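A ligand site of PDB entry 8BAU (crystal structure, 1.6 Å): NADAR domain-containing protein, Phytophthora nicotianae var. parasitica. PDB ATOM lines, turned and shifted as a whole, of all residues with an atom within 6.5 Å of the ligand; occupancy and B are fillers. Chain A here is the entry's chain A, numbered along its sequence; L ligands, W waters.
The backbone carbonyl oxygen (O) of Gly 80 is in hydrogen-bond range of a nitrogen (N3) of the ligand (3.0 Å). The side-chain carboxylate (OE2) of Glu 45 lies within hydrogen-bond range of an oxygen (O10) of the ligand, 2.6 Å away. The backbone carbonyl oxygen (O) of Arg 81 lies close to a nitrogen (N3) of the ligand (3.3 Å). An oxygen (O10) of the ligand sits at hydrogen-bond distance from the side-chain amide nitrogen of Asn 27 (2.7 Å). The side-chain carboxylate of Asp 88 sits at hydrogen-bond distance from an oxygen (O8) of the ligand (2.7 Å). An oxygen (O5) of the ligand is in salt-bridge range of the side-chain amino group (NZ) of Lys 52, 2.8 Å away. The guanidinium group (NH1) of Arg 95 lies within salt-bridge range of an oxygen (O1) of the ligand (2.7 Å). An oxygen (O5) of the ligand lies within hydrogen-bond range of the indole nitrogen (NE1) of Trp 91 (2.9 Å). The indole nitrogen of Trp 135 is in hydrogen-bond range of an oxygen (O1) of the ligand, 2.9 Å away. A nitrogen (N3) of the ligand lies within hydrogen-bond range of the backbone carbonyl oxygen (O) of Val 83. The guanidinium group of Arg 81 lies within salt-bridge range of an oxygen (O6) of the ligand (2.8 Å).
The backbone carbonyl oxygen (O) of Ile 134 sits at hydrogen-bond distance from the backbone NH (N) of Leu 173. The side-chain carboxylate (OE2) of Glu 127 sits close to the backbone NH (N) of Gly 136. The side-chain carboxylate of Asp 88 is in hydrogen-bond range of the side-chain hydroxyl of Tyr 86. The backbone NH (N) of Trp 135 is in hydrogen-bond range of the side-chain carboxylate (OD1) of Asp 132, at 2.9 Å. The side-chain amino group of Lys 52 sits close to the backbone carbonyl oxygen of Gly 80, at 3.4 Å. The backbone NH (N) of Phe 28 is in hydrogen-bond range of the side-chain hydroxyl (OG) of Ser 26 (2.9 Å). OD1 of Asn 27 sits at hydrogen-bond distance from OG of Ser 44, 2.6 Å away. The backbone carbonyl oxygen (O) of Trp 135 sits at hydrogen-bond distance from the backbone NH (N) of Leu 173, 3.3 Å away.
Merely in contact with the ligand: Phe 28, Phe 48, Met 49, Lys 77, Tyr 86, Met 99, Glu 127, Asp 132, Ile 134 and Leu 174. Within 4 Å of the ligand: Asn 27, Phe 28, Glu 45, Phe 48, Met 49, Lys 52, Lys 77, Gly 80, Arg 81, Val 83, Tyr 86, Asp 88, Trp 91, Arg 95, Met 99, Glu 127, Asp 132, Ile 134, Trp 135 and Leu 174. The nearest printed residue that does not touch the ligand is Gln 82 (4.1 Å).
Water W5 lies within hydrogen-bond range of an oxygen (O6) of the ligand, the side-chain amino group of Lys 52, the backbone carbonyl oxygen of Lys 77, the backbone NH of Arg 81 and the side-chain sulfur of Met 49. Water W3 bridges N1 of the ligand (2.6 Å) and O of Val 83 (3.3 Å). Water W8 lies within hydrogen-bond range of the side-chain carboxylate of Glu 127, the side-chain carboxylate of Asp 132 and an oxygen (O7) of the ligand. Water W6 lies within hydrogen-bond range of OD2 of Asp 132 (2.7 Å), O2 of the ligand (2.8 Å) and NZ of Lys 77 (2.9 Å). Water W4 lies within hydrogen-bond range of O7 of the ligand (2.8 Å), OE1 of Glu 127 (3.1 Å) and N of Asn 27 (3.2 Å). Water W9 lies within hydrogen-bond range of O of Arg 81 (2.8 Å) and N2 of the ligand (3.4 Å).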
ATOM      1  N   SER A  26     -24.485 -21.859 -16.319  1.00  0.00           N
ATOM      2  CA  SER A  26     -24.573 -22.041 -14.870  1.00  0.00           C
ATOM      3  C   SER A  26     -23.193 -22.007 -14.206  1.00  0.00           C
ATOM      4  O   SER A  26     -22.254 -22.672 -14.633  1.00  0.00           O
ATOM      5  CB  SER A  26     -25.225 -23.364 -14.552  1.00  0.00           C
ATOM      6  OG  SER A  26     -25.085 -23.591 -13.163  1.00  0.00           O
ATOM      7  N   ASN A  27     -23.053 -21.329 -13.061  1.00  0.00           N
ATOM      8  CA  ASN A  27     -21.809 -21.417 -12.330  1.00  0.00           C
ATOM      9  C   ASN A  27     -21.587 -22.776 -11.664  1.00  0.00           C
ATOM     10  O   ASN A  27     -20.456 -23.071 -11.229  1.00  0.00           O
ATOM     11  CB  ASN A  27     -21.666 -20.299 -11.291  1.00  0.00           C
ATOM     12  CG  ASN A  27     -21.419 -18.951 -11.930  1.00  0.00           C
ATOM     13  OD1 ASN A  27     -20.686 -18.868 -12.913  1.00  0.00           O
ATOM     14  ND2 ASN A  27     -21.858 -17.894 -11.238  1.00  0.00           N
ATOM     15  N   PHE A  28     -22.623 -23.627 -11.595  1.00  0.00           N
ATOM     16  CA  PHE A  28     -22.463 -24.998 -11.085  1.00  0.00           C
ATOM     17  C   PHE A  28     -21.916 -25.953 -12.165  1.00  0.00           C
ATOM     18  O   PHE A  28     -21.675 -27.132 -11.868  1.00  0.00           O
ATOM     19  CB  PHE A  28     -23.798 -25.542 -10.539  1.00  0.00           C
ATOM     20  CG  PHE A  28     -24.209 -25.110  -9.157  1.00  0.00           C
ATOM     21  CD1 PHE A  28     -23.801 -23.908  -8.570  1.00  0.00           C
ATOM     22  CD2 PHE A  28     -25.026 -25.934  -8.386  1.00  0.00           C
ATOM     23  CE1 PHE A  28     -24.184 -23.573  -7.277  1.00  0.00           C
ATOM     24  CE2 PHE A  28     -25.436 -25.596  -7.117  1.00  0.00           C
ATOM     25  CZ  PHE A  28     -24.953 -24.448  -6.518  1.00  0.00           C
ATOM     26  N   SER A  44     -16.877 -22.298 -11.670  1.00  0.00           N
ATOM     27  CA  SER A  44     -16.735 -20.859 -11.416  1.00  0.00           C
ATOM     28  C   SER A  44     -17.268 -20.591 -10.002  1.00  0.00           C
ATOM     29  O   SER A  44     -16.768 -19.729  -9.277  1.00  0.00           O
ATOM     30  CB  SER A  44     -17.389 -20.047 -12.465  1.00  0.00           C
ATOM     31  OG  SER A  44     -18.728 -20.520 -12.785  1.00  0.00           O
ATOM     32  N   GLU A  45     -18.290 -21.361  -9.609  1.00  0.00           N
ATOM     33  CA  GLU A  45     -18.812 -21.256  -8.249  1.00  0.00           C
ATOM     34  C   GLU A  45     -17.692 -21.352  -7.222  1.00  0.00           C
ATOM     35  O   GLU A  45     -17.650 -20.544  -6.289  1.00  0.00           O
ATOM     36  CB  GLU A  45     -19.880 -22.331  -8.012  1.00  0.00           C
ATOM     37  CG  GLU A  45     -20.644 -22.113  -6.731  1.00  0.00           C
ATOM     38  CD  GLU A  45     -21.735 -21.102  -6.840  1.00  0.00           C
ATOM     39  OE1 GLU A  45     -22.477 -20.859  -5.792  1.00  0.00           O
ATOM     40  OE2 GLU A  45     -21.863 -20.558  -7.944  1.00  0.00           O
ATOM     41  N   PHE A  48     -15.266 -18.313  -7.029  1.00  0.00           N
ATOM     42  CA  PHE A  48     -15.919 -17.171  -6.440  1.00  0.00           C
ATOM     43  C   PHE A  48     -15.999 -17.307  -4.907  1.00  0.00           C
ATOM     44  O   PHE A  48     -15.691 -16.359  -4.166  1.00  0.00           O
ATOM     45  CB  PHE A  48     -17.313 -17.049  -7.023  1.00  0.00           C
ATOM     46  CG  PHE A  48     -18.204 -15.974  -6.426  1.00  0.00           C
ATOM     47  CD1 PHE A  48     -18.159 -14.667  -6.873  1.00  0.00           C
ATOM     48  CD2 PHE A  48     -19.029 -16.253  -5.341  1.00  0.00           C
ATOM     49  CE1 PHE A  48     -19.078 -13.744  -6.434  1.00  0.00           C
ATOM     50  CE2 PHE A  48     -19.944 -15.343  -4.875  1.00  0.00           C
ATOM     51  CZ  PHE A  48     -19.902 -14.050  -5.362  1.00  0.00           C
ATOM     52  N   MET A  49     -16.321 -18.534  -4.427  1.00  0.00           N
ATOM     53  CA  MET A  49     -16.384 -18.750  -2.974  1.00  0.00           C
ATOM     54  C   MET A  49     -15.002 -18.698  -2.306  1.00  0.00           C
ATOM     55  O   MET A  49     -14.877 -18.138  -1.188  1.00  0.00           O
ATOM     56  CB  MET A  49     -17.054 -20.079  -2.645  1.00  0.00           C
ATOM     57  CG  MET A  49     -18.452 -20.141  -3.172  1.00  0.00           C
ATOM     58  SD  MET A  49     -19.536 -18.900  -2.463  1.00  0.00           S
ATOM     59  CE  MET A  49     -20.884 -18.862  -3.668  1.00  0.00           C
ATOM     60  N   LYS A  52     -14.212 -15.076  -1.839  1.00  0.00           N
ATOM     61  CA  LYS A  52     -14.928 -14.546  -0.678  1.00  0.00           C
ATOM     62  C   LYS A  52     -14.209 -14.848   0.643  1.00  0.00           C
ATOM     63  O   LYS A  52     -14.030 -13.942   1.461  1.00  0.00           O
ATOM     64  CB  LYS A  52     -16.391 -15.019  -0.599  1.00  0.00           C
ATOM     65  CG  LYS A  52     -17.220 -14.433   0.532  1.00  0.00           C
ATOM     66  CD  LYS A  52     -18.724 -14.392   0.245  1.00  0.00           C
ATOM     67  CE  LYS A  52     -19.306 -15.690  -0.186  1.00  0.00           C
ATOM     68  NZ  LYS A  52     -20.780 -15.684  -0.141  1.00  0.00           N
ATOM     69  N   PHE A  56     -12.383 -12.019   3.380  1.00  0.00           N
ATOM     70  CA  PHE A  56     -12.893 -11.811   4.726  1.00  0.00           C
ATOM     71  C   PHE A  56     -12.164 -12.619   5.822  1.00  0.00           C
ATOM     72  O   PHE A  56     -12.171 -12.205   6.981  1.00  0.00           O
ATOM     73  CB  PHE A  56     -14.420 -12.009   4.752  1.00  0.00           C
ATOM     74  CG  PHE A  56     -15.133 -11.023   3.892  1.00  0.00           C
ATOM     75  CD1 PHE A  56     -15.045  -9.657   4.131  1.00  0.00           C
ATOM     76  CD2 PHE A  56     -15.803 -11.419   2.740  1.00  0.00           C
ATOM     77  CE1 PHE A  56     -15.621  -8.716   3.286  1.00  0.00           C
ATOM     78  CE2 PHE A  56     -16.466 -10.502   1.944  1.00  0.00           C
ATOM     79  CZ  PHE A  56     -16.306  -9.144   2.154  1.00  0.00           C
ATOM     80  N   LYS A  77     -20.794 -23.236  -2.130  1.00  0.00           N
ATOM     81  CA  LYS A  77     -21.732 -22.161  -1.830  1.00  0.00           C
ATOM     82  C   LYS A  77     -22.041 -22.070  -0.337  1.00  0.00           C
ATOM     83  O   LYS A  77     -22.056 -20.962   0.295  1.00  0.00           O
ATOM     84  CB  LYS A  77     -22.971 -22.341  -2.673  1.00  0.00           C
ATOM     85  CG  LYS A  77     -23.903 -21.141  -2.594  1.00  0.00           C
ATOM     86  CD  LYS A  77     -25.129 -21.355  -3.370  1.00  0.00           C
ATOM     87  CE  LYS A  77     -26.018 -20.155  -3.263  1.00  0.00           C
ATOM     88  NZ  LYS A  77     -27.367 -20.477  -3.772  1.00  0.00           N
ATOM     89  N   LEU A  79     -20.311 -23.297   2.213  1.00  0.00           N
ATOM     90  CA  LEU A  79     -19.125 -22.777   2.866  1.00  0.00           C
ATOM     91  C   LEU A  79     -19.015 -21.272   2.729  1.00  0.00           C
ATOM     92  O   LEU A  79     -18.693 -20.562   3.706  1.00  0.00           O
ATOM     93  CB  LEU A  79     -17.884 -23.488   2.284  1.00  0.00           C
ATOM     94  CG  LEU A  79     -17.768 -24.956   2.667  1.00  0.00           C
ATOM     95  CD1 LEU A  79     -16.751 -25.668   1.811  1.00  0.00           C
ATOM     96  CD2 LEU A  79     -17.381 -25.112   4.137  1.00  0.00           C
ATOM     97  N   GLY A  80     -19.359 -20.763   1.526  1.00  0.00           N
ATOM     98  CA  GLY A  80     -19.284 -19.335   1.296  1.00  0.00           C
ATOM     99  C   GLY A  80     -20.246 -18.551   2.203  1.00  0.00           C
ATOM    100  O   GLY A  80     -19.920 -17.430   2.661  1.00  0.00           O
ATOM    101  N   ARG A  81     -21.403 -19.150   2.490  1.00  0.00           N
ATOM    102  CA  ARG A  81     -22.410 -18.499   3.321  1.00  0.00           C
ATOM    103  C   ARG A  81     -21.920 -18.467   4.769  1.00  0.00           C
ATOM    104  O   ARG A  81     -22.503 -17.722   5.555  1.00  0.00           O
ATOM    105  CB  ARG A  81     -23.780 -19.213   3.224  1.00  0.00           C
ATOM    106  CG  ARG A  81     -24.558 -18.919   1.945  1.00  0.00           C
ATOM    107  CD  ARG A  81     -24.741 -17.438   1.622  1.00  0.00           C
ATOM    108  NE  ARG A  81     -25.465 -17.239   0.418  1.00  0.00           N
ATOM    109  CZ  ARG A  81     -26.771 -17.274   0.286  1.00  0.00           C
ATOM    110  NH1 ARG A  81     -27.298 -17.069  -0.893  1.00  0.00           N
ATOM    111  NH2 ARG A  81     -27.561 -17.643   1.298  1.00  0.00           N
ATOM    112  N   GLN A  82     -20.952 -19.318   5.114  1.00  0.00           N
ATOM    113  CA  GLN A  82     -20.467 -19.462   6.475  1.00  0.00           C
ATOM    114  C   GLN A  82     -19.156 -18.703   6.697  1.00  0.00           C
ATOM    115  O   GLN A  82     -18.589 -18.697   7.815  1.00  0.00           O
ATOM    116  CB  GLN A  82     -20.342 -20.948   6.826  1.00  0.00           C
ATOM    117  CG  GLN A  82     -21.672 -21.644   6.869  1.00  0.00           C
ATOM    118  CD  GLN A  82     -21.476 -23.133   6.894  1.00  0.00           C
ATOM    119  OE1 GLN A  82     -20.365 -23.646   6.759  1.00  0.00           O
ATOM    120  NE2 GLN A  82     -22.567 -23.860   7.076  1.00  0.00           N
ATOM    121  N   VAL A  83     -18.645 -18.015   5.665  1.00  0.00           N
ATOM    122  CA  VAL A  83     -17.374 -17.336   5.786  1.00  0.00           C
ATOM    123  C   VAL A  83     -17.504 -16.283   6.894  1.00  0.00           C
ATOM    124  O   VAL A  83     -18.508 -15.545   6.943  1.00  0.00           O
ATOM    125  CB  VAL A  83     -16.909 -16.706   4.445  1.00  0.00           C
ATOM    126  CG1 VAL A  83     -15.887 -15.597   4.674  1.00  0.00           C
ATOM    127  CG2 VAL A  83     -16.278 -17.747   3.540  1.00  0.00           C
ATOM    128  N   GLU A  84     -16.495 -16.256   7.801  1.00  0.00           N
ATOM    129  CA  GLU A  84     -16.557 -15.339   8.948  1.00  0.00           C
ATOM    130  C   GLU A  84     -16.028 -13.940   8.594  1.00  0.00           C
ATOM    131  O   GLU A  84     -15.375 -13.736   7.597  1.00  0.00           O
ATOM    132  CB  GLU A  84     -15.824 -15.943  10.143  1.00  0.00           C
ATOM    133  CG  GLU A  84     -16.534 -17.179  10.639  1.00  0.00           C
ATOM    134  CD  GLU A  84     -15.729 -17.943  11.658  1.00  0.00           C
ATOM    135  OE1 GLU A  84     -15.837 -19.199  11.664  1.00  0.00           O
ATOM    136  OE2 GLU A  84     -14.962 -17.293  12.387  1.00  0.00           O
ATOM    137  N   TYR A  86     -17.730 -11.586   7.484  1.00  0.00           N
ATOM    138  CA  TYR A  86     -18.359 -11.162   6.236  1.00  0.00           C
ATOM    139  C   TYR A  86     -18.846  -9.718   6.362  1.00  0.00           C
ATOM    140  O   TYR A  86     -19.462  -9.363   7.340  1.00  0.00           O
ATOM    141  CB  TYR A  86     -19.512 -12.079   5.855  1.00  0.00           C
ATOM    142  CG  TYR A  86     -20.239 -11.671   4.599  1.00  0.00           C
ATOM    143  CD1 TYR A  86     -19.715 -11.930   3.338  1.00  0.00           C
ATOM    144  CD2 TYR A  86     -21.444 -10.974   4.651  1.00  0.00           C
ATOM    145  CE1 TYR A  86     -20.317 -11.467   2.166  1.00  0.00           C
ATOM    146  CE2 TYR A  86     -22.067 -10.534   3.487  1.00  0.00           C
ATOM    147  CZ  TYR A  86     -21.535 -10.829   2.227  1.00  0.00           C
ATOM    148  OH  TYR A  86     -22.172 -10.347   1.098  1.00  0.00           O
ATOM    149  N   ASP A  88     -21.184  -7.108   4.172  1.00  0.00           N
ATOM    150  CA  ASP A  88     -21.946  -7.110   2.929  1.00  0.00           C
ATOM    151  C   ASP A  88     -21.607  -5.924   2.057  1.00  0.00           C
ATOM    152  O   ASP A  88     -21.807  -5.924   0.840  1.00  0.00           O
ATOM    153  CB  ASP A  88     -23.457  -7.097   3.153  1.00  0.00           C
ATOM    154  CG  ASP A  88     -24.265  -7.537   1.953  1.00  0.00           C
ATOM    155  OD1 ASP A  88     -24.050  -8.674   1.478  1.00  0.00           O
ATOM    156  OD2 ASP A  88     -25.149  -6.783   1.540  1.00  0.00           O
ATOM    157  N   TRP A  91     -18.470  -6.765   0.266  1.00  0.00           N
ATOM    158  CA  TRP A  91     -18.690  -7.788  -0.778  1.00  0.00           C
ATOM    159  C   TRP A  91     -19.490  -7.230  -1.947  1.00  0.00           C
ATOM    160  O   TRP A  91     -19.217  -7.516  -3.128  1.00  0.00           O
ATOM    161  CB  TRP A  91     -19.244  -9.055  -0.174  1.00  0.00           C
ATOM    162  CG  TRP A  91     -19.195 -10.221  -1.126  1.00  0.00           C
ATOM    163  CD1 TRP A  91     -20.246 -11.013  -1.512  1.00  0.00           C
ATOM    164  CD2 TRP A  91     -18.020 -10.781  -1.707  1.00  0.00           C
ATOM    165  NE1 TRP A  91     -19.798 -12.021  -2.325  1.00  0.00           N
ATOM    166  CE2 TRP A  91     -18.456 -11.912  -2.464  1.00  0.00           C
ATOM    167  CE3 TRP A  91     -16.665 -10.429  -1.744  1.00  0.00           C
ATOM    168  CZ2 TRP A  91     -17.545 -12.723  -3.136  1.00  0.00           C
ATOM    169  CZ3 TRP A  91     -15.759 -11.280  -2.337  1.00  0.00           C
ATOM    170  CH2 TRP A  91     -16.217 -12.375  -3.112  1.00  0.00           C
ATOM    171  N   ALA A  92     -20.493  -6.435  -1.639  1.00  0.00           N
ATOM    172  CA  ALA A  92     -21.288  -5.879  -2.692  1.00  0.00           C
ATOM    173  C   ALA A  92     -20.471  -5.012  -3.657  1.00  0.00           C
ATOM    174  O   ALA A  92     -20.784  -4.915  -4.817  1.00  0.00           O
ATOM    175  CB  ALA A  92     -22.465  -5.157  -2.144  1.00  0.00           C
ATOM    176  N   ARG A  95     -17.958  -8.002  -5.558  1.00  0.00           N
ATOM    177  CA  ARG A  95     -18.315  -9.384  -5.950  1.00  0.00           C
ATOM    178  C   ARG A  95     -18.537  -9.532  -7.483  1.00  0.00           C
ATOM    179  O   ARG A  95     -18.229 -10.606  -8.050  1.00  0.00           O
ATOM    180  CB  ARG A  95     -19.520  -9.849  -5.132  1.00  0.00           C
ATOM    181  CG  ARG A  95     -20.825  -9.106  -5.396  1.00  0.00           C
ATOM    182  CD  ARG A  95     -21.899  -9.559  -4.407  1.00  0.00           C
ATOM    183  NE  ARG A  95     -23.101  -8.723  -4.391  1.00  0.00           N
ATOM    184  CZ  ARG A  95     -24.034  -8.843  -3.455  1.00  0.00           C
ATOM    185  NH1 ARG A  95     -23.959  -9.884  -2.633  1.00  0.00           N
ATOM    186  NH2 ARG A  95     -24.924  -7.856  -3.268  1.00  0.00           N
ATOM    187  N   MET A  99     -16.638 -12.280  -9.701  1.00  0.00           N
ATOM    188  CA  MET A  99     -17.312 -13.201 -10.605  1.00  0.00           C
ATOM    189  C   MET A  99     -16.798 -13.089 -12.031  1.00  0.00           C
ATOM    190  O   MET A  99     -16.656 -14.115 -12.696  1.00  0.00           O
ATOM    191  CB  MET A  99     -18.822 -12.994 -10.618  1.00  0.00           C
ATOM    192  CG  MET A  99     -19.563 -14.069 -11.402  1.00  0.00           C
ATOM    193  SD  MET A  99     -19.456 -15.691 -10.666  1.00  0.00           S
ATOM    194  CE  MET A  99     -20.555 -15.595  -9.262  1.00  0.00           C
ATOM    195  N   GLU A 127     -30.121 -14.947 -15.819  1.00  0.00           N
ATOM    196  CA  GLU A 127     -30.332 -16.150 -15.022  1.00  0.00           C
ATOM    197  C   GLU A 127     -31.721 -16.093 -14.389  1.00  0.00           C
ATOM    198  O   GLU A 127     -31.932 -15.371 -13.410  1.00  0.00           O
ATOM    199  CB  GLU A 127     -29.271 -16.330 -13.932  1.00  0.00           C
ATOM    200  CG  GLU A 127     -29.335 -17.742 -13.349  1.00  0.00           C
ATOM    201  CD  GLU A 127     -28.723 -17.898 -11.983  1.00  0.00           C
ATOM    202  OE1 GLU A 127     -28.068 -18.945 -11.789  1.00  0.00           O
ATOM    203  OE2 GLU A 127     -28.798 -16.945 -11.128  1.00  0.00           O
ATOM    204  N   ASP A 132     -32.821 -16.430  -6.437  1.00  0.00           N
ATOM    205  CA  ASP A 132     -31.674 -15.511  -6.384  1.00  0.00           C
ATOM    206  C   ASP A 132     -31.946 -14.255  -7.208  1.00  0.00           C
ATOM    207  O   ASP A 132     -31.911 -14.278  -8.451  1.00  0.00           O
ATOM    208  CB  ASP A 132     -30.433 -16.274  -6.838  1.00  0.00           C
ATOM    209  CG  ASP A 132     -29.126 -15.548  -6.623  1.00  0.00           C
ATOM    210  OD1 ASP A 132     -29.187 -14.328  -6.396  1.00  0.00           O
ATOM    211  OD2 ASP A 132     -28.095 -16.175  -6.791  1.00  0.00           O
ATOM    212  N   ILE A 134     -30.040 -11.463  -6.708  1.00  0.00           N
ATOM    213  CA  ILE A 134     -28.764 -10.778  -6.803  1.00  0.00           C
ATOM    214  C   ILE A 134     -28.014 -11.249  -8.064  1.00  0.00           C
ATOM    215  O   ILE A 134     -27.776 -10.479  -9.019  1.00  0.00           O
ATOM    216  CB  ILE A 134     -27.955 -10.995  -5.512  1.00  0.00           C
ATOM    217  CG1 ILE A 134     -28.711 -10.347  -4.324  1.00  0.00           C
ATOM    218  CG2 ILE A 134     -26.530 -10.468  -5.679  1.00  0.00           C
ATOM    219  CD1 ILE A 134     -28.075 -10.637  -2.982  1.00  0.00           C
ATOM    220  N   TRP A 135     -27.663 -12.538  -8.088  1.00  0.00           N
ATOM    221  CA  TRP A 135     -27.043 -13.111  -9.270  1.00  0.00           C
ATOM    222  C   TRP A 135     -28.011 -13.418 -10.419  1.00  0.00           C
ATOM    223  O   TRP A 135     -27.670 -13.364 -11.588  1.00  0.00           O
ATOM    224  CB  TRP A 135     -26.164 -14.299  -8.860  1.00  0.00           C
ATOM    225  CG  TRP A 135     -25.034 -13.827  -7.984  1.00  0.00           C
ATOM    226  CD1 TRP A 135     -25.059 -13.713  -6.619  1.00  0.00           C
ATOM    227  CD2 TRP A 135     -23.856 -13.135  -8.439  1.00  0.00           C
ATOM    228  NE1 TRP A 135     -23.941 -13.060  -6.181  1.00  0.00           N
ATOM    229  CE2 TRP A 135     -23.170 -12.708  -7.272  1.00  0.00           C
ATOM    230  CE3 TRP A 135     -23.281 -12.923  -9.699  1.00  0.00           C
ATOM    231  CZ2 TRP A 135     -21.972 -11.975  -7.352  1.00  0.00           C
ATOM    232  CZ3 TRP A 135     -22.113 -12.196  -9.763  1.00  0.00           C
ATOM    233  CH2 TRP A 135     -21.459 -11.743  -8.615  1.00  0.00           C
ATOM    234  N   GLY A 136     -29.244 -13.687 -10.096  1.00  0.00           N
ATOM    235  CA  GLY A 136     -30.307 -13.857 -11.083  1.00  0.00           C
ATOM    236  C   GLY A 136     -31.339 -12.734 -11.031  1.00  0.00           C
ATOM    237  O   GLY A 136     -31.191 -11.719 -10.340  1.00  0.00           O
ATOM    238  N   LEU A 173     -26.715 -10.199 -11.732  1.00  0.00           N
ATOM    239  CA  LEU A 173     -25.287  -9.959 -11.790  1.00  0.00           C
ATOM    240  C   LEU A 173     -24.611 -11.059 -12.608  1.00  0.00           C
ATOM    241  O   LEU A 173     -23.630 -10.771 -13.308  1.00  0.00           O
ATOM    242  CB  LEU A 173     -24.648  -9.864 -10.413  1.00  0.00           C
ATOM    243  CG  LEU A 173     -25.081  -8.648  -9.578  1.00  0.00           C
ATOM    244  CD1 LEU A 173     -24.254  -8.620  -8.329  1.00  0.00           C
ATOM    245  CD2 LEU A 173     -25.014  -7.350 -10.373  1.00  0.00           C
ATOM    246  N   LEU A 174     -25.122 -12.311 -12.585  1.00  0.00           N
ATOM    247  CA  LEU A 174     -24.501 -13.354 -13.391  1.00  0.00           C
ATOM    248  C   LEU A 174     -24.721 -13.120 -14.875  1.00  0.00           C
ATOM    249  O   LEU A 174     -23.783 -13.286 -15.680  1.00  0.00           O
ATOM    250  CB  LEU A 174     -25.022 -14.747 -13.020  1.00  0.00           C
ATOM    251  CG  LEU A 174     -24.445 -15.928 -13.794  1.00  0.00           C
ATOM    252  CD1 LEU A 174     -22.927 -15.938 -13.739  1.00  0.00           C
ATOM    253  CD2 LEU A 174     -24.965 -17.262 -13.178  1.00  0.00           C
HETATM  254  N1  LIG L   1     -22.150 -14.312   5.852  1.00  0.00           N
HETATM  255  C1  LIG L   1     -23.259 -13.548   5.820  1.00  0.00           C
HETATM  256  N2  LIG L   1     -24.146 -13.333   4.824  1.00  0.00           N
HETATM  257  C2  LIG L   1     -23.670 -13.800   3.675  1.00  0.00           C
HETATM  258  C3  LIG L   1     -22.504 -14.502   3.501  1.00  0.00           C
HETATM  259  C4  LIG L   1     -21.696 -14.708   4.634  1.00  0.00           C
HETATM  260  N3  LIG L   1     -20.487 -15.239   4.580  1.00  0.00           N
HETATM  261  N4  LIG L   1     -22.341 -14.758   2.109  1.00  0.00           N
HETATM  262  C5  LIG L   1     -23.437 -14.317   1.585  1.00  0.00           C
HETATM  263  N5  LIG L   1     -24.246 -13.717   2.429  1.00  0.00           N
HETATM  264  P1  LIG L   1     -23.092 -13.587  -2.607  1.00  0.00           P
HETATM  265  P2  LIG L   1     -24.412 -16.270  -2.962  1.00  0.00           P
HETATM  266  C6  LIG L   1     -25.531 -13.142   2.134  1.00  0.00           C
HETATM  267  O1  LIG L   1     -23.189 -12.372  -3.505  1.00  0.00           O
HETATM  268  O2  LIG L   1     -25.870 -16.199  -3.164  1.00  0.00           O
HETATM  269  C7  LIG L   1     -25.246 -18.915  -7.066  1.00  0.00           C
HETATM  270  O3  LIG L   1     -25.204 -20.140  -7.718  1.00  0.00           O
HETATM  271  C8  LIG L   1     -25.552 -11.634   2.032  1.00  0.00           C
HETATM  272  O4  LIG L   1     -26.858 -11.131   2.236  1.00  0.00           O
HETATM  273  O5  LIG L   1     -21.816 -14.152  -2.195  1.00  0.00           O
HETATM  274  O6  LIG L   1     -23.716 -16.623  -1.691  1.00  0.00           O
HETATM  275  C9  LIG L   1     -25.020 -17.740  -8.070  1.00  0.00           C
HETATM  276  O7  LIG L   1     -25.486 -18.007  -9.382  1.00  0.00           O
HETATM  277  C10 LIG L   1     -25.171 -11.396   0.543  1.00  0.00           C
HETATM  278  O8  LIG L   1     -25.660 -10.174  -0.001  1.00  0.00           O
HETATM  279  O9  LIG L   1     -23.932 -14.758  -3.364  1.00  0.00           O
HETATM  280  C11 LIG L   1     -23.565 -17.397  -7.901  1.00  0.00           C
HETATM  281  O10 LIG L   1     -22.676 -18.195  -8.674  1.00  0.00           O
HETATM  282  C12 LIG L   1     -25.980 -12.540  -0.110  1.00  0.00           C
HETATM  283  O11 LIG L   1     -25.951 -13.628   0.870  1.00  0.00           O
HETATM  284  C13 LIG L   1     -23.356 -17.644  -6.406  1.00  0.00           C
HETATM  285  O12 LIG L   1     -24.166 -18.843  -6.104  1.00  0.00           O
HETATM  286  C14 LIG L   1     -25.442 -13.045  -1.448  1.00  0.00           C
HETATM  287  O13 LIG L   1     -24.067 -13.373  -1.382  1.00  0.00           O
HETATM  288  C15 LIG L   1     -23.887 -16.573  -5.453  1.00  0.00           C
HETATM  289  O14 LIG L   1     -23.600 -17.037  -4.102  1.00  0.00           O
HETATM  290  O   HOH W   1     -26.476  -7.429  -0.951  1.00  0.00           O
HETATM  291  O   HOH W   2     -27.519 -14.326  -3.987  1.00  0.00           O
HETATM  292  O   HOH W   3     -21.373 -14.777   8.288  1.00  0.00           O
HETATM  293  O   HOH W   4     -25.280 -20.175 -11.122  1.00  0.00           O
HETATM  294  O   HOH W   5     -21.996 -18.178  -0.517  1.00  0.00           O
HETATM  295  O   HOH W   6     -27.714 -17.689  -4.611  1.00  0.00           O
HETATM  296  O   HOH W   7     -28.133  -9.180   0.420  1.00  0.00           O
HETATM  297  O   HOH W   8     -28.175 -17.744  -8.845  1.00  0.00           O
HETATM  298  O   HOH W   9     -25.031 -16.488   5.699  1.00  0.00           O
